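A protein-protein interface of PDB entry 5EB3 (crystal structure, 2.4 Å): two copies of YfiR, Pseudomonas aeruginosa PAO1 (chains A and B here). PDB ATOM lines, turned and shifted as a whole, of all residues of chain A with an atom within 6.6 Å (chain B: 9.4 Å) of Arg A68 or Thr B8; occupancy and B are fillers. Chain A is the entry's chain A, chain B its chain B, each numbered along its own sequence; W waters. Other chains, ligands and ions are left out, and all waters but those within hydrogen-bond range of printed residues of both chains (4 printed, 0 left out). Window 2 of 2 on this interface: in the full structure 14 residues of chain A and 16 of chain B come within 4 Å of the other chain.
Among the printed residues, pairs that only touch across the chains: Glu A66 with Thr B8 (3.3 Å), Gly A43 with Glu B46 (3.4 Å), Arg A68 with Ile B10 (3.5 Å), Ala A69 with Ile B10 (3.6 Å), Arg A68 with Thr B8 (3.6 Å), Glu A66 with Glu B11 (3.6 Å) and Arg A67 with Ile B10 (3.7 Å).
Arg A68 touches just these residues of chain B: Thr B8 and Ile B10.
Of chain B, only Ile B10 comes within 4 Å of Ala A69.
Of the printed residues of chain A, Asp B49 touches Arg A67.
Of the printed residues of chain A, Glu B46 touches Gly A43 (3.4 Å) and Arg A67 (3.4 Å).
Printed residues of chain B within 4 Å of Gly A43: Glu B46.
Gln A38 touches none of the printed residues of chain B.
The nearest residue of chain A that does not touch Thr B8 is Ala A69 (6.0 Å).
The nearest printed residue of chain A that does not touch Asp B49 is Glu A66 (7.0 Å).
The backbone NH (N) of Val A41 lies within hydrogen-bond range of the backbone carbonyl oxygen (O) of Glu A66 (3.0 Å).
The side-chain sulfur (SG) of Cys A40 is disulfide-bonded to the side-chain sulfur (SG) of Cys A79.
O of Ile B10 is in hydrogen-bond range of OG of Ser B14 (2.8 Å).
OE2 of Glu A66 is in salt-bridge range of NH2 of Arg A68, at 2.7 Å.
O of Val A41 sits at hydrogen-bond distance from N of Arg A68 (2.9 Å).
N of Thr B8 lies within hydrogen-bond range of OE2 of Glu B11 (3.2 Å).
The guanidinium group (NE) of Arg A67 lies close to the backbone carbonyl oxygen (O) of Glu B46 (3.4 Å).
O of Arg A67 sits at hydrogen-bond distance from OG1 of Thr B8 (3.1 Å).
NH1 of Arg A67 is in salt-bridge range of OD1 of Asp B49, at 2.9 Å.
Water W2 lies within hydrogen-bond range of OE1 of Glu B46 (2.6 Å) and N of Val A70 (3.1 Å).
Water W3 lies within hydrogen-bond range of the backbone carbonyl oxygen of Arg A68 (2.7 Å), the side-chain carboxylate of Glu B46 (3.0 Å) and the backbone NH of Gly A43 (3.2 Å).
Water W1 bridges OE1 of Glu B11 and N of Arg A67.
Water W4 bridges the guanidinium group (NH1) of Arg A67 (3.4 Å) and the side-chain carboxylate (OD1) of Asp B49 (3.4 Å).
Of the 17 printed residues of chain A, 5 touch a printed residue of chain B.
Hydrophobic or aromatic side chains of chain A within 4 Å of the printed part of chain B: Ala A69.
Among the printed residues, Asp or Glu carboxylates within 4 Å of a Lys or Arg side-chain nitrogen of the other chain: Arg A67 with Asp B49 (2.9 Å).
No position is printed for both chains.
Of the 10 pairs that touch across the chains among the printed residues, none has its exchanged pair printed and touching as well.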
ATOM      1  N   GLN A  38      -4.278   0.087  13.434  1.00  0.00           N
ATOM      2  CA  GLN A  38      -2.997  -0.575  13.178  1.00  0.00           C
ATOM      3  C   GLN A  38      -2.027  -0.390  14.332  1.00  0.00           C
ATOM      4  O   GLN A  38      -1.691   0.742  14.699  1.00  0.00           O
ATOM      5  CB  GLN A  38      -2.368  -0.073  11.878  1.00  0.00           C
ATOM      6  CG  GLN A  38      -3.152  -0.467  10.626  1.00  0.00           C
ATOM      7  CD  GLN A  38      -3.173  -1.964  10.402  1.00  0.00           C
ATOM      8  OE1 GLN A  38      -2.349  -2.697  10.940  1.00  0.00           O
ATOM      9  NE2 GLN A  38      -4.119  -2.427   9.602  1.00  0.00           N
ATOM     10  N   LEU A  39      -1.592  -1.511  14.902  1.00  0.00           N
ATOM     11  CA  LEU A  39      -0.675  -1.505  16.033  1.00  0.00           C
ATOM     12  C   LEU A  39       0.652  -2.081  15.574  1.00  0.00           C
ATOM     13  O   LEU A  39       0.704  -3.126  14.922  1.00  0.00           O
ATOM     14  CB  LEU A  39      -1.232  -2.342  17.189  1.00  0.00           C
ATOM     15  CG  LEU A  39      -0.487  -2.322  18.530  1.00  0.00           C
ATOM     16  CD1 LEU A  39      -1.412  -2.707  19.652  1.00  0.00           C
ATOM     17  CD2 LEU A  39       0.692  -3.260  18.541  1.00  0.00           C
ATOM     18  N   CYS A  40       1.728  -1.392  15.925  1.00  0.00           N
ATOM     19  CA  CYS A  40       3.061  -1.829  15.572  1.00  0.00           C
ATOM     20  C   CYS A  40       3.853  -2.076  16.833  1.00  0.00           C
ATOM     21  O   CYS A  40       3.959  -1.191  17.692  1.00  0.00           O
ATOM     22  CB  CYS A  40       3.749  -0.758  14.742  1.00  0.00           C
ATOM     23  SG  CYS A  40       2.918  -0.511  13.193  1.00  0.00           S
ATOM     24  N   VAL A  41       4.382  -3.291  16.955  1.00  0.00           N
ATOM     25  CA  VAL A  41       5.273  -3.630  18.056  1.00  0.00           C
ATOM     26  C   VAL A  41       6.692  -3.401  17.545  1.00  0.00           C
ATOM     27  O   VAL A  41       7.080  -3.931  16.495  1.00  0.00           O
ATOM     28  CB  VAL A  41       5.076  -5.088  18.510  1.00  0.00           C
ATOM     29  CG1 VAL A  41       6.102  -5.463  19.542  1.00  0.00           C
ATOM     30  CG2 VAL A  41       3.683  -5.276  19.077  1.00  0.00           C
ATOM     31  N   VAL A  42       7.454  -2.583  18.262  1.00  0.00           N
ATOM     32  CA  VAL A  42       8.758  -2.158  17.780  1.00  0.00           C
ATOM     33  C   VAL A  42       9.853  -2.409  18.810  1.00  0.00           C
ATOM     34  O   VAL A  42       9.797  -1.893  19.931  1.00  0.00           O
ATOM     35  CB  VAL A  42       8.741  -0.663  17.413  1.00  0.00           C
ATOM     36  CG1 VAL A  42      10.115  -0.220  16.957  1.00  0.00           C
ATOM     37  CG2 VAL A  42       7.742  -0.414  16.322  1.00  0.00           C
ATOM     38  N   GLY A  43      10.856  -3.191  18.424  1.00  0.00           N
ATOM     39  CA  GLY A  43      11.936  -3.523  19.336  1.00  0.00           C
ATOM     40  C   GLY A  43      11.596  -4.782  20.107  1.00  0.00           C
ATOM     41  O   GLY A  43      10.486  -5.296  19.982  1.00  0.00           O
ATOM     42  N   GLU A  66       1.348  -6.167  14.288  1.00  0.00           N
ATOM     43  CA  GLU A  66       2.533  -6.849  13.777  1.00  0.00           C
ATOM     44  C   GLU A  66       3.809  -6.160  14.245  1.00  0.00           C
ATOM     45  O   GLU A  66       3.803  -4.960  14.540  1.00  0.00           O
ATOM     46  CB  GLU A  66       2.497  -6.952  12.254  1.00  0.00           C
ATOM     47  CG  GLU A  66       2.484  -5.626  11.522  1.00  0.00           C
ATOM     48  CD  GLU A  66       2.175  -5.808  10.047  1.00  0.00           C
ATOM     49  OE1 GLU A  66       1.422  -6.748   9.708  1.00  0.00           O
ATOM     50  OE2 GLU A  66       2.685  -5.019   9.221  1.00  0.00           O
ATOM     51  N   ARG A  67       4.898  -6.919  14.331  1.00  0.00           N
ATOM     52  CA  ARG A  67       6.180  -6.329  14.679  1.00  0.00           C
ATOM     53  C   ARG A  67       6.719  -5.590  13.461  1.00  0.00           C
ATOM     54  O   ARG A  67       6.523  -6.024  12.322  1.00  0.00           O
ATOM     55  CB  ARG A  67       7.193  -7.389  15.132  1.00  0.00           C
ATOM     56  CG  ARG A  67       6.608  -8.569  15.873  1.00  0.00           C
ATOM     57  CD  ARG A  67       7.701  -9.348  16.600  1.00  0.00           C
ATOM     58  NE  ARG A  67       8.090  -8.659  17.821  1.00  0.00           N
ATOM     59  CZ  ARG A  67       7.847  -9.108  19.049  1.00  0.00           C
ATOM     60  NH1 ARG A  67       7.234 -10.279  19.240  1.00  0.00           N
ATOM     61  NH2 ARG A  67       8.240  -8.381  20.093  1.00  0.00           N
ATOM     62  N   ARG A  68       7.384  -4.464  13.703  1.00  0.00           N
ATOM     63  CA  ARG A  68       8.049  -3.727  12.635  1.00  0.00           C
ATOM     64  C   ARG A  68       9.403  -3.266  13.112  1.00  0.00           C
ATOM     65  O   ARG A  68       9.631  -3.130  14.312  1.00  0.00           O
ATOM     66  CB  ARG A  68       7.237  -2.509  12.204  1.00  0.00           C
ATOM     67  CG  ARG A  68       5.961  -2.837  11.463  1.00  0.00           C
ATOM     68  CD  ARG A  68       5.380  -1.564  10.862  1.00  0.00           C
ATOM     69  NE  ARG A  68       4.214  -1.836  10.030  1.00  0.00           N
ATOM     70  CZ  ARG A  68       4.274  -2.410   8.832  1.00  0.00           C
ATOM     71  NH1 ARG A  68       5.451  -2.793   8.332  1.00  0.00           N
ATOM     72  NH2 ARG A  68       3.159  -2.612   8.137  1.00  0.00           N
ATOM     73  N   ALA A  69      10.294  -3.013  12.162  1.00  0.00           N
ATOM     74  CA  ALA A  69      11.669  -2.653  12.473  1.00  0.00           C
ATOM     75  C   ALA A  69      11.766  -1.255  13.059  1.00  0.00           C
ATOM     76  O   ALA A  69      11.037  -0.347  12.656  1.00  0.00           O
ATOM     77  CB  ALA A  69      12.542  -2.766  11.229  1.00  0.00           C
ATOM     78  N   VAL A  70      12.685  -1.101  14.008  1.00  0.00           N
ATOM     79  CA  VAL A  70      13.026   0.193  14.585  1.00  0.00           C
ATOM     80  C   VAL A  70      13.324   1.255  13.527  1.00  0.00           C
ATOM     81  O   VAL A  70      12.863   2.392  13.623  1.00  0.00           O
ATOM     82  CB  VAL A  70      14.256   0.056  15.488  1.00  0.00           C
ATOM     83  CG1 VAL A  70      14.852   1.410  15.770  1.00  0.00           C
ATOM     84  CG2 VAL A  70      13.878  -0.622  16.779  1.00  0.00           C
ATOM     85  N   ASP A  71      14.085   0.879  12.509  1.00  0.00           N
ATOM     86  CA  ASP A  71      14.519   1.846  11.507  1.00  0.00           C
ATOM     87  C   ASP A  71      13.560   1.982  10.328  1.00  0.00           C
ATOM     88  O   ASP A  71      13.928   2.542   9.300  1.00  0.00           O
ATOM     89  CB  ASP A  71      15.928   1.511  11.007  1.00  0.00           C
ATOM     90  CG  ASP A  71      16.093   0.038  10.651  1.00  0.00           C
ATOM     91  OD1 ASP A  71      15.085  -0.654  10.398  1.00  0.00           O
ATOM     92  OD2 ASP A  71      17.248  -0.433  10.611  1.00  0.00           O
ATOM     93  N   ASN A  72      12.339   1.474  10.463  1.00  0.00           N
ATOM     94  CA  ASN A  72      11.347   1.704   9.417  1.00  0.00           C
ATOM     95  C   ASN A  72      10.912   3.165   9.434  1.00  0.00           C
ATOM     96  O   ASN A  72      10.263   3.618  10.378  1.00  0.00           O
ATOM     97  CB  ASN A  72      10.145   0.768   9.570  1.00  0.00           C
ATOM     98  CG  ASN A  72       9.183   0.855   8.394  1.00  0.00           C
ATOM     99  OD1 ASN A  72       9.027   1.908   7.770  1.00  0.00           O
ATOM    100  ND2 ASN A  72       8.529  -0.257   8.089  1.00  0.00           N
ATOM    101  N   ASP A  74       8.693   4.663   7.947  1.00  0.00           N
ATOM    102  CA  ASP A  74       7.275   4.930   7.743  1.00  0.00           C
ATOM    103  C   ASP A  74       6.402   4.473   8.890  1.00  0.00           C
ATOM    104  O   ASP A  74       5.198   4.296   8.711  1.00  0.00           O
ATOM    105  CB  ASP A  74       6.805   4.296   6.438  1.00  0.00           C
ATOM    106  CG  ASP A  74       7.600   4.779   5.259  1.00  0.00           C
ATOM    107  OD1 ASP A  74       7.848   5.997   5.200  1.00  0.00           O
ATOM    108  OD2 ASP A  74       8.002   3.948   4.417  1.00  0.00           O
ATOM    109  N   LEU A  75       7.004   4.289  10.064  1.00  0.00           N
ATOM    110  CA  LEU A  75       6.246   3.899  11.251  1.00  0.00           C
ATOM    111  C   LEU A  75       5.072   4.847  11.489  1.00  0.00           C
ATOM    112  O   LEU A  75       3.959   4.403  11.790  1.00  0.00           O
ATOM    113  CB  LEU A  75       7.140   3.880  12.490  1.00  0.00           C
ATOM    114  CG  LEU A  75       8.200   2.791  12.611  1.00  0.00           C
ATOM    115  CD1 LEU A  75       8.888   2.876  13.956  1.00  0.00           C
ATOM    116  CD2 LEU A  75       7.562   1.444  12.431  1.00  0.00           C
ATOM    117  N   LEU A  78       2.378   3.954   8.867  1.00  0.00           N
ATOM    118  CA  LEU A  78       1.899   2.573   8.905  1.00  0.00           C
ATOM    119  C   LEU A  78       1.208   2.188  10.213  1.00  0.00           C
ATOM    120  O   LEU A  78       0.498   1.184  10.268  1.00  0.00           O
ATOM    121  CB  LEU A  78       3.073   1.621   8.666  1.00  0.00           C
ATOM    122  CG  LEU A  78       3.754   1.737   7.307  1.00  0.00           C
ATOM    123  CD1 LEU A  78       5.121   1.064   7.298  1.00  0.00           C
ATOM    124  CD2 LEU A  78       2.862   1.121   6.269  1.00  0.00           C
ATOM    125  N   CYS A  79       1.412   2.979  11.262  1.00  0.00           N
ATOM    126  CA  CYS A  79       0.948   2.592  12.585  1.00  0.00           C
ATOM    127  C   CYS A  79       0.043   3.643  13.212  1.00  0.00           C
ATOM    128  O   CYS A  79       0.345   4.839  13.161  1.00  0.00           O
ATOM    129  CB  CYS A  79       2.150   2.356  13.499  1.00  0.00           C
ATOM    130  SG  CYS A  79       3.504   1.390  12.764  1.00  0.00           S
ATOM    131  N   ARG B   7       4.137  -9.725   4.841  1.00  0.00           N
ATOM    132  CA  ARG B   7       5.195 -10.224   5.722  1.00  0.00           C
ATOM    133  C   ARG B   7       6.286  -9.162   5.976  1.00  0.00           C
ATOM    134  O   ARG B   7       7.071  -8.845   5.082  1.00  0.00           O
ATOM    135  CB  ARG B   7       5.816 -11.488   5.115  1.00  0.00           C
ATOM    136  CG  ARG B   7       6.340 -12.527   6.108  1.00  0.00           C
ATOM    137  CD  ARG B   7       7.536 -13.242   5.486  1.00  0.00           C
ATOM    138  NE  ARG B   7       7.733 -14.624   5.919  1.00  0.00           N
ATOM    139  CZ  ARG B   7       8.724 -15.400   5.480  1.00  0.00           C
ATOM    140  NH1 ARG B   7       9.600 -14.925   4.604  1.00  0.00           N
ATOM    141  NH2 ARG B   7       8.844 -16.648   5.906  1.00  0.00           N
ATOM    142  N   THR B   8       6.328  -8.621   7.197  1.00  0.00           N
ATOM    143  CA  THR B   8       7.350  -7.636   7.596  1.00  0.00           C
ATOM    144  C   THR B   8       8.774  -8.216   7.606  1.00  0.00           C
ATOM    145  O   THR B   8       8.956  -9.439   7.590  1.00  0.00           O
ATOM    146  CB  THR B   8       7.062  -7.023   9.005  1.00  0.00           C
ATOM    147  OG1 THR B   8       7.065  -8.054  10.007  1.00  0.00           O
ATOM    148  CG2 THR B   8       5.729  -6.294   9.033  1.00  0.00           C
ATOM    149  N   SER B   9       9.781  -7.343   7.647  1.00  0.00           N
ATOM    150  CA  SER B   9      11.159  -7.820   7.687  1.00  0.00           C
ATOM    151  C   SER B   9      11.448  -8.455   9.042  1.00  0.00           C
ATOM    152  O   SER B   9      12.322  -9.312   9.150  1.00  0.00           O
ATOM    153  CB  SER B   9      12.170  -6.712   7.359  1.00  0.00           C
ATOM    154  OG  SER B   9      12.356  -5.817   8.444  1.00  0.00           O
ATOM    155  N   ILE B  10      10.703  -8.059  10.070  1.00  0.00           N
ATOM    156  CA  ILE B  10      10.857  -8.715  11.363  1.00  0.00           C
ATOM    157  C   ILE B  10      10.324 -10.143  11.268  1.00  0.00           C
ATOM    158  O   ILE B  10      10.879 -11.066  11.881  1.00  0.00           O
ATOM    159  CB  ILE B  10      10.145  -7.971  12.501  1.00  0.00           C
ATOM    160  CG1 ILE B  10      10.631  -6.525  12.584  1.00  0.00           C
ATOM    161  CG2 ILE B  10      10.396  -8.677  13.827  1.00  0.00           C
ATOM    162  CD1 ILE B  10      12.126  -6.395  12.843  1.00  0.00           C
ATOM    163  N   GLU B  11       9.264 -10.333  10.487  1.00  0.00           N
ATOM    164  CA  GLU B  11       8.709 -11.673  10.335  1.00  0.00           C
ATOM    165  C   GLU B  11       9.620 -12.579   9.504  1.00  0.00           C
ATOM    166  O   GLU B  11       9.840 -13.737   9.872  1.00  0.00           O
ATOM    167  CB  GLU B  11       7.287 -11.631   9.775  1.00  0.00           C
ATOM    168  CG  GLU B  11       6.271 -11.072  10.771  1.00  0.00           C
ATOM    169  CD  GLU B  11       5.043 -10.482  10.100  1.00  0.00           C
ATOM    170  OE1 GLU B  11       4.336  -9.688  10.755  1.00  0.00           O
ATOM    171  OE2 GLU B  11       4.780 -10.815   8.924  1.00  0.00           O
ATOM    172  N   GLN B  12      10.148 -12.054   8.398  1.00  0.00           N
ATOM    173  CA  GLN B  12      11.103 -12.803   7.580  1.00  0.00           C
ATOM    174  C   GLN B  12      12.258 -13.270   8.461  1.00  0.00           C
ATOM    175  O   GLN B  12      12.557 -14.462   8.530  1.00  0.00           O
ATOM    176  CB  GLN B  12      11.634 -11.948   6.416  1.00  0.00           C
ATOM    177  CG  GLN B  12      10.715 -11.848   5.183  1.00  0.00           C
ATOM    178  CD  GLN B  12      10.892 -10.543   4.391  1.00  0.00           C
ATOM    179  OE1 GLN B  12      11.796  -9.745   4.661  1.00  0.00           O
ATOM    180  NE2 GLN B  12      10.017 -10.326   3.411  1.00  0.00           N
ATOM    181  N   ARG B  13      12.883 -12.324   9.156  1.00  0.00           N
ATOM    182  CA  ARG B  13      13.999 -12.624  10.041  1.00  0.00           C
ATOM    183  C   ARG B  13      13.644 -13.641  11.107  1.00  0.00           C
ATOM    184  O   ARG B  13      14.448 -14.529  11.409  1.00  0.00           O
ATOM    185  CB  ARG B  13      14.487 -11.351  10.714  1.00  0.00           C
ATOM    186  CG  ARG B  13      15.445 -10.546   9.870  1.00  0.00           C
ATOM    187  CD  ARG B  13      15.442  -9.119  10.327  1.00  0.00           C
ATOM    188  NE  ARG B  13      16.482  -8.329   9.688  1.00  0.00           N
ATOM    189  CZ  ARG B  13      16.609  -7.019   9.855  1.00  0.00           C
ATOM    190  NH1 ARG B  13      15.753  -6.366  10.636  1.00  0.00           N
ATOM    191  NH2 ARG B  13      17.586  -6.369   9.244  1.00  0.00           N
ATOM    192  N   SER B  14      12.455 -13.498  11.685  1.00  0.00           N
ATOM    193  CA  SER B  14      11.995 -14.410  12.727  1.00  0.00           C
ATOM    194  C   SER B  14      11.978 -15.840  12.219  1.00  0.00           C
ATOM    195  O   SER B  14      12.397 -16.770  12.920  1.00  0.00           O
ATOM    196  CB  SER B  14      10.602 -14.015  13.212  1.00  0.00           C
ATOM    197  OG  SER B  14      10.664 -12.879  14.044  1.00  0.00           O
ATOM    198  N   ASN B  15      11.497 -16.015  10.995  1.00  0.00           N
ATOM    199  CA  ASN B  15      11.499 -17.342  10.407  1.00  0.00           C
ATOM    200  C   ASN B  15      12.922 -17.827  10.152  1.00  0.00           C
ATOM    201  O   ASN B  15      13.246 -18.971  10.425  1.00  0.00           O
ATOM    202  CB  ASN B  15      10.578 -17.404   9.183  1.00  0.00           C
ATOM    203  CG  ASN B  15       9.094 -17.337   9.581  1.00  0.00           C
ATOM    204  OD1 ASN B  15       8.716 -17.749  10.689  1.00  0.00           O
ATOM    205  ND2 ASN B  15       8.256 -16.807   8.690  1.00  0.00           N
ATOM    206  N   ALA B  16      13.788 -16.933   9.692  1.00  0.00           N
ATOM    207  CA  ALA B  16      15.196 -17.276   9.521  1.00  0.00           C
ATOM    208  C   ALA B  16      15.832 -17.682  10.857  1.00  0.00           C
ATOM    209  O   ALA B  16      16.573 -18.670  10.925  1.00  0.00           O
ATOM    210  CB  ALA B  16      15.944 -16.124   8.902  1.00  0.00           C
ATOM    211  N   GLU B  46      12.894  -9.768  19.835  1.00  0.00           N
ATOM    212  CA  GLU B  46      12.277  -9.250  18.617  1.00  0.00           C
ATOM    213  C   GLU B  46      11.910 -10.371  17.664  1.00  0.00           C
ATOM    214  O   GLU B  46      10.968 -10.259  16.878  1.00  0.00           O
ATOM    215  CB  GLU B  46      13.264  -8.355  17.876  1.00  0.00           C
ATOM    216  CG  GLU B  46      12.888  -6.913  17.798  1.00  0.00           C
ATOM    217  CD  GLU B  46      13.896  -6.114  17.010  1.00  0.00           C
ATOM    218  OE1 GLU B  46      13.460  -5.365  16.115  1.00  0.00           O
ATOM    219  OE2 GLU B  46      15.115  -6.233  17.284  1.00  0.00           O
ATOM    220  N   TYR B  47      12.683 -11.449  17.713  1.00  0.00           N
ATOM    221  CA  TYR B  47      12.655 -12.409  16.634  1.00  0.00           C
ATOM    222  C   TYR B  47      12.264 -13.825  17.086  1.00  0.00           C
ATOM    223  O   TYR B  47      12.526 -14.813  16.387  1.00  0.00           O
ATOM    224  CB  TYR B  47      14.021 -12.416  15.945  1.00  0.00           C
ATOM    225  CG  TYR B  47      14.481 -11.081  15.386  1.00  0.00           C
ATOM    226  CD1 TYR B  47      13.941 -10.562  14.213  1.00  0.00           C
ATOM    227  CD2 TYR B  47      15.497 -10.367  16.003  1.00  0.00           C
ATOM    228  CE1 TYR B  47      14.385  -9.350  13.693  1.00  0.00           C
ATOM    229  CE2 TYR B  47      15.945  -9.156  15.494  1.00  0.00           C
ATOM    230  CZ  TYR B  47      15.389  -8.654  14.343  1.00  0.00           C
ATOM    231  OH  TYR B  47      15.847  -7.451  13.840  1.00  0.00           O
ATOM    232  N   ASP B  49       9.119 -14.985  17.667  1.00  0.00           N
ATOM    233  CA  ASP B  49       7.727 -15.381  17.424  1.00  0.00           C
ATOM    234  C   ASP B  49       7.604 -16.680  16.648  1.00  0.00           C
ATOM    235  O   ASP B  49       6.678 -17.453  16.876  1.00  0.00           O
ATOM    236  CB  ASP B  49       6.943 -14.290  16.714  1.00  0.00           C
ATOM    237  CG  ASP B  49       6.745 -13.079  17.570  1.00  0.00           C
ATOM    238  OD1 ASP B  49       7.012 -13.169  18.786  1.00  0.00           O
ATOM    239  OD2 ASP B  49       6.325 -12.036  17.025  1.00  0.00           O
HETATM  240  O   HOH W   1       4.591  -9.838  13.518  1.00  0.00           O
HETATM  241  O   HOH W   2      14.436  -3.585  14.535  1.00  0.00           O
HETATM  242  O   HOH W   3      10.521  -5.108  15.850  1.00  0.00           O
HETATM  243  O   HOH W   4       9.966 -12.091  20.043  1.00  0.00           O
